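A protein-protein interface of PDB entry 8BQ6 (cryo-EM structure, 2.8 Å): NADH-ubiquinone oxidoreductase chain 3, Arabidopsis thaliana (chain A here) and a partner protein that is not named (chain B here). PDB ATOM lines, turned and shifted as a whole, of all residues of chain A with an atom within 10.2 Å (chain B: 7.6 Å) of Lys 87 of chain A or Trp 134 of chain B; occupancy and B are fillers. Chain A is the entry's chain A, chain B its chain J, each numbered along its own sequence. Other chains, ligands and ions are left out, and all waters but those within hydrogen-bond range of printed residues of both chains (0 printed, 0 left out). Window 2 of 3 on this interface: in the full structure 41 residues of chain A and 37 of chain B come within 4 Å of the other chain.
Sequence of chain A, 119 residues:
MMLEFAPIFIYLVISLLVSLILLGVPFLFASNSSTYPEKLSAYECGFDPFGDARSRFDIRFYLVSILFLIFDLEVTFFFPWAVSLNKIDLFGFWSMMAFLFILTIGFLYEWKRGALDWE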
ATOM      1  N   FME A   1       7.817   1.044 -15.387  1.00  0.00           N
ATOM      2  CN  FME A   1       6.909   0.654 -14.428  1.00  0.00           C
ATOM      3  O1  FME A   1       7.192   0.433 -13.240  1.00  0.00           O
ATOM      4  CA  FME A   1       9.227   1.253 -15.189  1.00  0.00           C
ATOM      5  CB  FME A   1       9.921   1.757 -16.472  1.00  0.00           C
ATOM      6  CG  FME A   1       9.548   0.925 -17.668  1.00  0.00           C
ATOM      7  SD  FME A   1       9.685  -0.771 -17.175  1.00  0.00           S
ATOM      8  CE  FME A   1      11.421  -0.983 -17.085  1.00  0.00           C
ATOM      9  C   FME A   1       9.571   2.256 -14.091  1.00  0.00           C
ATOM     10  O   FME A   1       8.988   3.475 -14.250  1.00  0.00           O
ATOM     11  N   MET A   2      10.605   1.934 -13.320  1.00  0.00           N
ATOM     12  CA  MET A   2      11.097   2.809 -12.261  1.00  0.00           C
ATOM     13  C   MET A   2      12.452   3.395 -12.618  1.00  0.00           C
ATOM     14  O   MET A   2      13.110   4.002 -11.776  1.00  0.00           O
ATOM     15  CB  MET A   2      11.211   2.053 -10.938  1.00  0.00           C
ATOM     16  CG  MET A   2       9.943   1.390 -10.477  1.00  0.00           C
ATOM     17  SD  MET A   2       8.877   2.549  -9.610  1.00  0.00           S
ATOM     18  CE  MET A   2       7.723   2.952 -10.915  1.00  0.00           C
ATOM     19  N   PRO A  80      -6.144   8.458  -7.817  1.00  0.00           N
ATOM     20  CA  PRO A  80      -6.544   7.270  -8.572  1.00  0.00           C
ATOM     21  C   PRO A  80      -7.886   7.487  -9.285  1.00  0.00           C
ATOM     22  O   PRO A  80      -8.002   7.070 -10.385  1.00  0.00           O
ATOM     23  CB  PRO A  80      -6.643   6.144  -7.528  1.00  0.00           C
ATOM     24  CG  PRO A  80      -5.922   6.667  -6.315  1.00  0.00           C
ATOM     25  CD  PRO A  80      -6.083   8.168  -6.383  1.00  0.00           C
ATOM     26  N   TRP A  81      -8.838   8.164  -8.646  1.00  0.00           N
ATOM     27  CA  TRP A  81     -10.178   8.399  -9.238  1.00  0.00           C
ATOM     28  C   TRP A  81     -10.053   9.203 -10.530  1.00  0.00           C
ATOM     29  O   TRP A  81     -10.684   8.820 -11.514  1.00  0.00           O
ATOM     30  CB  TRP A  81     -11.059   9.114  -8.208  1.00  0.00           C
ATOM     31  CG  TRP A  81     -12.478   9.341  -8.621  1.00  0.00           C
ATOM     32  CD1 TRP A  81     -13.471   8.412  -8.693  1.00  0.00           C
ATOM     33  CD2 TRP A  81     -13.074  10.599  -8.975  1.00  0.00           C
ATOM     34  NE1 TRP A  81     -14.640   9.000  -9.090  1.00  0.00           N
ATOM     35  CE2 TRP A  81     -14.429  10.341  -9.268  1.00  0.00           C
ATOM     36  CE3 TRP A  81     -12.597  11.909  -9.082  1.00  0.00           C
ATOM     37  CZ2 TRP A  81     -15.311  11.348  -9.655  1.00  0.00           C
ATOM     38  CZ3 TRP A  81     -13.470  12.903  -9.464  1.00  0.00           C
ATOM     39  CH2 TRP A  81     -14.806  12.622  -9.746  1.00  0.00           C
ATOM     40  N   ALA A  82      -9.264  10.274 -10.505  1.00  0.00           N
ATOM     41  CA  ALA A  82      -9.109  11.154 -11.680  1.00  0.00           C
ATOM     42  C   ALA A  82      -8.454  10.371 -12.813  1.00  0.00           C
ATOM     43  O   ALA A  82      -8.879  10.561 -13.959  1.00  0.00           O
ATOM     44  CB  ALA A  82      -8.292  12.356 -11.308  1.00  0.00           C
ATOM     45  N   VAL A  83      -7.471   9.517 -12.501  1.00  0.00           N
ATOM     46  CA  VAL A  83      -6.914   8.773 -13.633  1.00  0.00           C
ATOM     47  C   VAL A  83      -7.773   7.589 -14.057  1.00  0.00           C
ATOM     48  O   VAL A  83      -7.575   7.064 -15.159  1.00  0.00           O
ATOM     49  CB  VAL A  83      -5.480   8.273 -13.369  1.00  0.00           C
ATOM     50  CG1 VAL A  83      -4.571   9.438 -12.990  1.00  0.00           C
ATOM     51  CG2 VAL A  83      -5.465   7.183 -12.324  1.00  0.00           C
ATOM     52  N   SER A  84      -8.727   7.155 -13.232  1.00  0.00           N
ATOM     53  CA  SER A  84      -9.540   5.984 -13.536  1.00  0.00           C
ATOM     54  C   SER A  84     -10.960   6.315 -13.965  1.00  0.00           C
ATOM     55  O   SER A  84     -11.755   5.394 -14.169  1.00  0.00           O
ATOM     56  CB  SER A  84      -9.596   5.052 -12.324  1.00  0.00           C
ATOM     57  OG  SER A  84      -8.362   5.040 -11.635  1.00  0.00           O
ATOM     58  N   LEU A  85     -11.298   7.599 -14.095  1.00  0.00           N
ATOM     59  CA  LEU A  85     -12.679   7.977 -14.387  1.00  0.00           C
ATOM     60  C   LEU A  85     -13.199   7.336 -15.669  1.00  0.00           C
ATOM     61  O   LEU A  85     -14.382   6.984 -15.744  1.00  0.00           O
ATOM     62  CB  LEU A  85     -12.785   9.499 -14.471  1.00  0.00           C
ATOM     63  CG  LEU A  85     -13.302  10.244 -13.240  1.00  0.00           C
ATOM     64  CD1 LEU A  85     -13.344  11.727 -13.535  1.00  0.00           C
ATOM     65  CD2 LEU A  85     -14.674   9.747 -12.823  1.00  0.00           C
ATOM     66  N   ASN A  86     -12.341   7.160 -16.678  1.00  0.00           N
ATOM     67  CA  ASN A  86     -12.801   6.627 -17.957  1.00  0.00           C
ATOM     68  C   ASN A  86     -13.184   5.153 -17.884  1.00  0.00           C
ATOM     69  O   ASN A  86     -13.885   4.667 -18.776  1.00  0.00           O
ATOM     70  CB  ASN A  86     -11.738   6.825 -19.039  1.00  0.00           C
ATOM     71  CG  ASN A  86     -10.411   6.183 -18.687  1.00  0.00           C
ATOM     72  OD1 ASN A  86      -9.820   6.473 -17.648  1.00  0.00           O
ATOM     73  ND2 ASN A  86      -9.933   5.304 -19.558  1.00  0.00           N
ATOM     74  N   LYS A  87     -12.746   4.432 -16.856  1.00  0.00           N
ATOM     75  CA  LYS A  87     -13.146   3.040 -16.702  1.00  0.00           C
ATOM     76  C   LYS A  87     -14.260   2.838 -15.688  1.00  0.00           C
ATOM     77  O   LYS A  87     -15.141   2.005 -15.916  1.00  0.00           O
ATOM     78  CB  LYS A  87     -11.940   2.179 -16.314  1.00  0.00           C
ATOM     79  CG  LYS A  87     -11.062   1.818 -17.499  1.00  0.00           C
ATOM     80  CD  LYS A  87      -9.802   1.099 -17.074  1.00  0.00           C
ATOM     81  CE  LYS A  87      -9.069   1.894 -16.028  1.00  0.00           C
ATOM     82  NZ  LYS A  87      -7.654   2.130 -16.395  1.00  0.00           N
ATOM     83  N   ILE A  88     -14.258   3.590 -14.585  1.00  0.00           N
ATOM     84  CA  ILE A  88     -15.253   3.379 -13.538  1.00  0.00           C
ATOM     85  C   ILE A  88     -16.613   3.966 -13.891  1.00  0.00           C
ATOM     86  O   ILE A  88     -17.624   3.539 -13.322  1.00  0.00           O
ATOM     87  CB  ILE A  88     -14.766   3.959 -12.203  1.00  0.00           C
ATOM     88  CG1 ILE A  88     -14.487   5.456 -12.344  1.00  0.00           C
ATOM     89  CG2 ILE A  88     -13.525   3.224 -11.739  1.00  0.00           C
ATOM     90  CD1 ILE A  88     -13.853   6.072 -11.136  1.00  0.00           C
ATOM     91  N   ASP A  89     -16.660   4.949 -14.782  1.00  0.00           N
ATOM     92  CA  ASP A  89     -17.907   5.457 -15.387  1.00  0.00           C
ATOM     93  C   ASP A  89     -18.787   6.073 -14.291  1.00  0.00           C
ATOM     94  O   ASP A  89     -18.288   6.836 -13.451  1.00  0.00           O
ATOM     95  CB  ASP A  89     -18.570   4.355 -16.175  1.00  0.00           C
ATOM     96  CG  ASP A  89     -19.616   4.882 -17.130  1.00  0.00           C
ATOM     97  OD1 ASP A  89     -19.670   6.113 -17.328  1.00  0.00           O
ATOM     98  OD2 ASP A  89     -20.400   4.073 -17.663  1.00  0.00           O
ATOM     99  N   LEU A  90     -20.088   5.771 -14.281  1.00  0.00           N
ATOM    100  CA  LEU A  90     -21.018   6.478 -13.405  1.00  0.00           C
ATOM    101  C   LEU A  90     -20.980   5.936 -11.985  1.00  0.00           C
ATOM    102  O   LEU A  90     -21.152   6.694 -11.023  1.00  0.00           O
ATOM    103  CB  LEU A  90     -22.431   6.389 -13.968  1.00  0.00           C
ATOM    104  CG  LEU A  90     -22.730   7.438 -15.033  1.00  0.00           C
ATOM    105  CD1 LEU A  90     -24.108   7.214 -15.613  1.00  0.00           C
ATOM    106  CD2 LEU A  90     -22.616   8.823 -14.434  1.00  0.00           C
ATOM    107  N   PHE A  91     -20.826   4.621 -11.841  1.00  0.00           N
ATOM    108  CA  PHE A  91     -20.737   4.021 -10.488  1.00  0.00           C
ATOM    109  C   PHE A  91     -19.585   4.680  -9.719  1.00  0.00           C
ATOM    110  O   PHE A  91     -19.827   5.122  -8.588  1.00  0.00           O
ATOM    111  CB  PHE A  91     -20.608   2.496 -10.558  1.00  0.00           C
ATOM    112  CG  PHE A  91     -20.974   1.771  -9.291  1.00  0.00           C
ATOM    113  CD1 PHE A  91     -20.084   1.695  -8.232  1.00  0.00           C
ATOM    114  CD2 PHE A  91     -22.210   1.162  -9.158  1.00  0.00           C
ATOM    115  CE1 PHE A  91     -20.426   1.031  -7.067  1.00  0.00           C
ATOM    116  CE2 PHE A  91     -22.550   0.492  -7.995  1.00  0.00           C
ATOM    117  CZ  PHE A  91     -21.658   0.429  -6.951  1.00  0.00           C
ATOM    118  N   GLY A  92     -18.389   4.751 -10.312  1.00  0.00           N
ATOM    119  CA  GLY A  92     -17.256   5.343  -9.621  1.00  0.00           C
ATOM    120  C   GLY A  92     -17.468   6.810  -9.306  1.00  0.00           C
ATOM    121  O   GLY A  92     -17.107   7.289  -8.222  1.00  0.00           O
ATOM    122  N   PHE A  93     -18.076   7.540 -10.244  1.00  0.00           N
ATOM    123  CA  PHE A  93     -18.363   8.949 -10.019  1.00  0.00           C
ATOM    124  C   PHE A  93     -19.244   9.141  -8.792  1.00  0.00           C
ATOM    125  O   PHE A  93     -18.956   9.978  -7.929  1.00  0.00           O
ATOM    126  CB  PHE A  93     -19.028   9.545 -11.260  1.00  0.00           C
ATOM    127  CG  PHE A  93     -19.504  10.948 -11.066  1.00  0.00           C
ATOM    128  CD1 PHE A  93     -18.638  12.009 -11.221  1.00  0.00           C
ATOM    129  CD2 PHE A  93     -20.812  11.205 -10.702  1.00  0.00           C
ATOM    130  CE1 PHE A  93     -19.069  13.298 -11.030  1.00  0.00           C
ATOM    131  CE2 PHE A  93     -21.246  12.495 -10.510  1.00  0.00           C
ATOM    132  CZ  PHE A  93     -20.373  13.541 -10.675  1.00  0.00           C
ATOM    133  N   GLY B 129       1.246  -9.105 -22.145  1.00  0.00           N
ATOM    134  CA  GLY B 129       0.996  -8.218 -21.028  1.00  0.00           C
ATOM    135  C   GLY B 129       1.576  -6.825 -21.165  1.00  0.00           C
ATOM    136  O   GLY B 129       1.169  -5.929 -20.422  1.00  0.00           O
ATOM    137  N   VAL B 131       1.593  -4.793 -23.958  1.00  0.00           N
ATOM    138  CA  VAL B 131       1.061  -3.947 -25.024  1.00  0.00           C
ATOM    139  C   VAL B 131       0.502  -2.649 -24.456  1.00  0.00           C
ATOM    140  O   VAL B 131       0.824  -1.555 -24.936  1.00  0.00           O
ATOM    141  CB  VAL B 131      -0.006  -4.714 -25.825  1.00  0.00           C
ATOM    142  CG1 VAL B 131      -0.794  -3.760 -26.701  1.00  0.00           C
ATOM    143  CG2 VAL B 131       0.638  -5.796 -26.666  1.00  0.00           C
ATOM    144  N   ARG B 132      -0.352  -2.751 -23.438  1.00  0.00           N
ATOM    145  CA  ARG B 132      -0.938  -1.603 -22.739  1.00  0.00           C
ATOM    146  C   ARG B 132      -0.820  -1.917 -21.252  1.00  0.00           C
ATOM    147  O   ARG B 132      -1.704  -2.548 -20.668  1.00  0.00           O
ATOM    148  CB  ARG B 132      -2.388  -1.363 -23.151  1.00  0.00           C
ATOM    149  CG  ARG B 132      -3.066  -0.204 -22.418  1.00  0.00           C
ATOM    150  CD  ARG B 132      -4.535  -0.058 -22.812  1.00  0.00           C
ATOM    151  NE  ARG B 132      -5.212   0.987 -22.052  1.00  0.00           N
ATOM    152  CZ  ARG B 132      -6.426   1.445 -22.331  1.00  0.00           C
ATOM    153  NH1 ARG B 132      -7.140   0.951 -23.329  1.00  0.00           N
ATOM    154  NH2 ARG B 132      -6.932   2.432 -21.595  1.00  0.00           N
ATOM    155  N   SER B 133       0.282  -1.485 -20.648  1.00  0.00           N
ATOM    156  CA  SER B 133       0.513  -1.731 -19.233  1.00  0.00           C
ATOM    157  C   SER B 133      -0.167  -0.672 -18.374  1.00  0.00           C
ATOM    158  O   SER B 133      -0.382   0.462 -18.809  1.00  0.00           O
ATOM    159  CB  SER B 133       2.004  -1.747 -18.939  1.00  0.00           C
ATOM    160  OG  SER B 133       2.636  -0.624 -19.534  1.00  0.00           O
ATOM    161  N   TRP B 134      -0.494  -1.055 -17.144  1.00  0.00           N
ATOM    162  CA  TRP B 134      -1.205  -0.204 -16.203  1.00  0.00           C
ATOM    163  C   TRP B 134      -0.236   0.318 -15.154  1.00  0.00           C
ATOM    164  O   TRP B 134       0.630  -0.420 -14.677  1.00  0.00           O
ATOM    165  CB  TRP B 134      -2.320  -0.981 -15.498  1.00  0.00           C
ATOM    166  CG  TRP B 134      -3.577  -1.151 -16.279  1.00  0.00           C
ATOM    167  CD1 TRP B 134      -3.721  -1.090 -17.631  1.00  0.00           C
ATOM    168  CD2 TRP B 134      -4.879  -1.418 -15.747  1.00  0.00           C
ATOM    169  NE1 TRP B 134      -5.033  -1.302 -17.977  1.00  0.00           N
ATOM    170  CE2 TRP B 134      -5.764  -1.506 -16.837  1.00  0.00           C
ATOM    171  CE3 TRP B 134      -5.381  -1.591 -14.455  1.00  0.00           C
ATOM    172  CZ2 TRP B 134      -7.121  -1.758 -16.675  1.00  0.00           C
ATOM    173  CZ3 TRP B 134      -6.727  -1.843 -14.296  1.00  0.00           C
ATOM    174  CH2 TRP B 134      -7.582  -1.924 -15.399  1.00  0.00           C
ATOM    175  N   THR B 135      -0.392   1.581 -14.778  1.00  0.00           N
ATOM    176  CA  THR B 135       0.395   2.077 -13.664  1.00  0.00           C
ATOM    177  C   THR B 135      -0.209   1.585 -12.350  1.00  0.00           C
ATOM    178  O   THR B 135      -1.327   1.066 -12.305  1.00  0.00           O
ATOM    179  CB  THR B 135       0.463   3.603 -13.680  1.00  0.00           C
ATOM    180  OG1 THR B 135      -0.858   4.145 -13.743  1.00  0.00           O
ATOM    181  CG2 THR B 135       1.222   4.073 -14.903  1.00  0.00           C
ATOM    182  N   ASN B 136       0.564   1.735 -11.274  1.00  0.00           N
ATOM    183  CA  ASN B 136       0.054   1.442  -9.939  1.00  0.00           C
ATOM    184  C   ASN B 136      -1.185   2.276  -9.640  1.00  0.00           C
ATOM    185  O   ASN B 136      -2.157   1.792  -9.039  1.00  0.00           O
ATOM    186  CB  ASN B 136       1.163   1.711  -8.919  1.00  0.00           C
ATOM    187  CG  ASN B 136       0.857   1.152  -7.553  1.00  0.00           C
ATOM    188  OD1 ASN B 136       1.329   1.670  -6.544  1.00  0.00           O
ATOM    189  ND2 ASN B 136       0.056   0.099  -7.509  1.00  0.00           N
ATOM    190  N   LEU B 137      -1.177   3.525 -10.104  1.00  0.00           N
ATOM    191  CA  LEU B 137      -2.272   4.446  -9.842  1.00  0.00           C
ATOM    192  C   LEU B 137      -3.575   3.951 -10.460  1.00  0.00           C
ATOM    193  O   LEU B 137      -4.597   3.844  -9.773  1.00  0.00           O
ATOM    194  CB  LEU B 137      -1.896   5.827 -10.372  1.00  0.00           C
ATOM    195  CG  LEU B 137      -2.742   7.028  -9.982  1.00  0.00           C
ATOM    196  CD1 LEU B 137      -2.991   7.012  -8.501  1.00  0.00           C
ATOM    197  CD2 LEU B 137      -2.021   8.291 -10.385  1.00  0.00           C
ATOM    198  N   GLU B 138      -3.561   3.627 -11.754  1.00  0.00           N
ATOM    199  CA  GLU B 138      -4.816   3.234 -12.386  1.00  0.00           C
ATOM    200  C   GLU B 138      -5.225   1.812 -12.026  1.00  0.00           C
ATOM    201  O   GLU B 138      -6.424   1.512 -12.001  1.00  0.00           O
ATOM    202  CB  GLU B 138      -4.744   3.410 -13.901  1.00  0.00           C
ATOM    203  CG  GLU B 138      -3.511   2.884 -14.555  1.00  0.00           C
ATOM    204  CD  GLU B 138      -3.258   3.557 -15.883  1.00  0.00           C
ATOM    205  OE1 GLU B 138      -2.810   2.871 -16.822  1.00  0.00           O
ATOM    206  OE2 GLU B 138      -3.515   4.774 -15.991  1.00  0.00           O
ATOM    207  N   THR B 139      -4.267   0.940 -11.711  1.00  0.00           N
ATOM    208  CA  THR B 139      -4.621  -0.382 -11.203  1.00  0.00           C
ATOM    209  C   THR B 139      -5.366  -0.285  -9.876  1.00  0.00           C
ATOM    210  O   THR B 139      -6.350  -0.999  -9.657  1.00  0.00           O
ATOM    211  CB  THR B 139      -3.370  -1.248 -11.062  1.00  0.00           C
ATOM    212  OG1 THR B 139      -2.635  -1.231 -12.292  1.00  0.00           O
ATOM    213  CG2 THR B 139      -3.741  -2.676 -10.722  1.00  0.00           C
ATOM    214  N   LEU B 140      -4.910   0.590  -8.973  1.00  0.00           N
ATOM    215  CA  LEU B 140      -5.636   0.782  -7.717  1.00  0.00           C
ATOM    216  C   LEU B 140      -6.974   1.486  -7.940  1.00  0.00           C
ATOM    217  O   LEU B 140      -7.994   1.125  -7.326  1.00  0.00           O
ATOM    218  CB  LEU B 140      -4.773   1.574  -6.740  1.00  0.00           C
ATOM    219  CG  LEU B 140      -5.189   1.646  -5.273  1.00  0.00           C
ATOM    220  CD1 LEU B 140      -5.508   0.273  -4.716  1.00  0.00           C
ATOM    221  CD2 LEU B 140      -4.088   2.313  -4.476  1.00  0.00           C
ATOM    222  N   GLY B 141      -6.990   2.498  -8.812  1.00  0.00           N
ATOM    223  CA  GLY B 141      -8.206   3.247  -9.067  1.00  0.00           C
ATOM    224  C   GLY B 141      -9.273   2.453  -9.782  1.00  0.00           C
ATOM    225  O   GLY B 141     -10.449   2.827  -9.729  1.00  0.00           O
ATOM    226  N   ASN B 142      -8.888   1.370 -10.456  1.00  0.00           N
ATOM    227  CA  ASN B 142      -9.858   0.463 -11.054  1.00  0.00           C
ATOM    228  C   ASN B 142     -10.691  -0.278 -10.013  1.00  0.00           C
ATOM    229  O   ASN B 142     -11.800  -0.723 -10.326  1.00  0.00           O
ATOM    230  CB  ASN B 142      -9.119  -0.530 -11.947  1.00  0.00           C
ATOM    231  CG  ASN B 142     -10.050  -1.423 -12.723  1.00  0.00           C
ATOM    232  OD1 ASN B 142     -10.854  -0.955 -13.526  1.00  0.00           O
ATOM    233  ND2 ASN B 142      -9.945  -2.722 -12.489  1.00  0.00           N
ATOM    234  N   LEU B 143     -10.187  -0.422  -8.789  1.00  0.00           N
ATOM    235  CA  LEU B 143     -10.858  -1.192  -7.751  1.00  0.00           C
ATOM    236  C   LEU B 143     -11.471  -0.354  -6.646  1.00  0.00           C
ATOM    237  O   LEU B 143     -12.513  -0.739  -6.113  1.00  0.00           O
ATOM    238  CB  LEU B 143      -9.885  -2.178  -7.100  1.00  0.00           C
ATOM    239  CG  LEU B 143      -9.239  -3.216  -8.006  1.00  0.00           C
ATOM    240  CD1 LEU B 143      -8.312  -4.087  -7.185  1.00  0.00           C
ATOM    241  CD2 LEU B 143     -10.311  -4.038  -8.680  1.00  0.00           C
ATOM    242  N   THR B 146     -15.379   0.979  -7.157  1.00  0.00           N
ATOM    243  CA  THR B 146     -16.443   0.151  -7.779  1.00  0.00           C
ATOM    244  C   THR B 146     -16.586  -1.161  -7.004  1.00  0.00           C
ATOM    245  O   THR B 146     -17.561  -1.283  -6.265  1.00  0.00           O
ATOM    246  CB  THR B 146     -16.175  -0.042  -9.279  1.00  0.00           C
ATOM    247  OG1 THR B 146     -14.778  -0.263  -9.484  1.00  0.00           O
ATOM    248  CG2 THR B 146     -16.632   1.134 -10.110  1.00  0.00           C
ATOM    249  N   TYR B 147     -15.621  -2.068  -7.127  1.00  0.00           N
ATOM    250  CA  TYR B 147     -15.726  -3.415  -6.505  1.00  0.00           C
ATOM    251  C   TYR B 147     -15.620  -3.321  -4.982  1.00  0.00           C
ATOM    252  O   TYR B 147     -16.237  -4.152  -4.318  1.00  0.00           O
ATOM    253  CB  TYR B 147     -14.723  -4.357  -7.184  1.00  0.00           C
ATOM    254  CG  TYR B 147     -14.962  -4.403  -8.669  1.00  0.00           C
ATOM    255  CD1 TYR B 147     -16.003  -5.152  -9.188  1.00  0.00           C
ATOM    256  CD2 TYR B 147     -14.219  -3.628  -9.545  1.00  0.00           C
ATOM    257  CE1 TYR B 147     -16.273  -5.168 -10.544  1.00  0.00           C
ATOM    258  CE2 TYR B 147     -14.481  -3.625 -10.903  1.00  0.00           C
ATOM    259  CZ  TYR B 147     -15.511  -4.400 -11.403  1.00  0.00           C
ATOM    260  OH  TYR B 147     -15.790  -4.409 -12.735  1.00  0.00           O
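The backbone carbonyl oxygen (O) of Pro 80 of chain A lies within hydrogen-bond range of the side-chain hydroxyl (OG) of Ser 84 of chain A (2.4 Å).
OD1 of Asn 86 of chain A lies close to O of Val 83 of chain A, at 3.4 Å.
The backbone carbonyl oxygen of Asn 142 of chain B is in hydrogen-bond range of the side-chain hydroxyl of Thr 146 of chain B (3.1 Å).
N of Pro 80 of chain A touches CD1 of Leu 137 of chain B (3.5 Å).
Pro 80 of chain A touches Gly 141 of chain B.
Val 83 of chain A touches Leu 137 of chain B (CG2 to CG, 3.6 Å).
Gly 141 of chain B touches Ser 84 of chain A.
Ser 84 of chain A touches Asn 142 of chain B (OG to N, 3.9 Å).
NZ of Lys 87 of chain A touches CZ2 of Trp 134 of chain B, at 3.9 Å.
Ile 88 of chain A touches Gly 141 of chain B (CG2 to O, 3.7 Å).
CG2 of Thr 146 of chain B touches CB of Ile 88 of chain A, 3.98 Å away.
Phe 91 of chain A touches Thr 146 of chain B.
Printed residues of chain B within 4 Å of Val 83 of chain A: Leu 137 (3.6 Å).
Of the printed residues of chain B, Lys 87 of chain A touches Trp 134.
Printed residues of chain B within 4 Å of Ile 88 of chain A: Gly 141 (3.7 Å) and Thr 146 (3.98 Å).
No residue of chain A comes within 4 Å of Ser 133 of chain B.
Trp 134 of chain B touches just one residue of chain A: Lys 87 (3.9 Å).
Thr 139 of chain B touches none of the printed residues of chain A.
Of the printed residues of chain A, Thr 146 of chain B touches Ile 88 (3.98 Å) and Phe 91 (3.8 Å).
The nearest residue of chain A that does not touch Trp 134 of chain B is FME 1 of chain A (6.4 Å).
Of the 16 printed residues of chain A, 6 touch a printed residue of chain B.
Printed residues of chain A that touch a printed residue of chain B: Pro 80, Val 83, Ser 84, Lys 87, Ile 88 and Phe 91.
Of the 16 printed residues of chain B, 5 touch a printed residue of chain A.
Printed residues of chain B that touch a printed residue of chain A: Trp 134, Leu 137, Gly 141, Asn 142 and Thr 146.
Hydrophobic or aromatic side chains of chain B that line the printed part of chain A: Trp 134 and Leu 137.
Along chain B the printed residues that touch a printed residue of chain A span positions 134 to 146.
Among the printed residues, 9 pairs touch across the chains.
Among the printed residues, no Asp or Glu carboxylate lies within 4 Å of a Lys or Arg side-chain nitrogen of the other chain.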
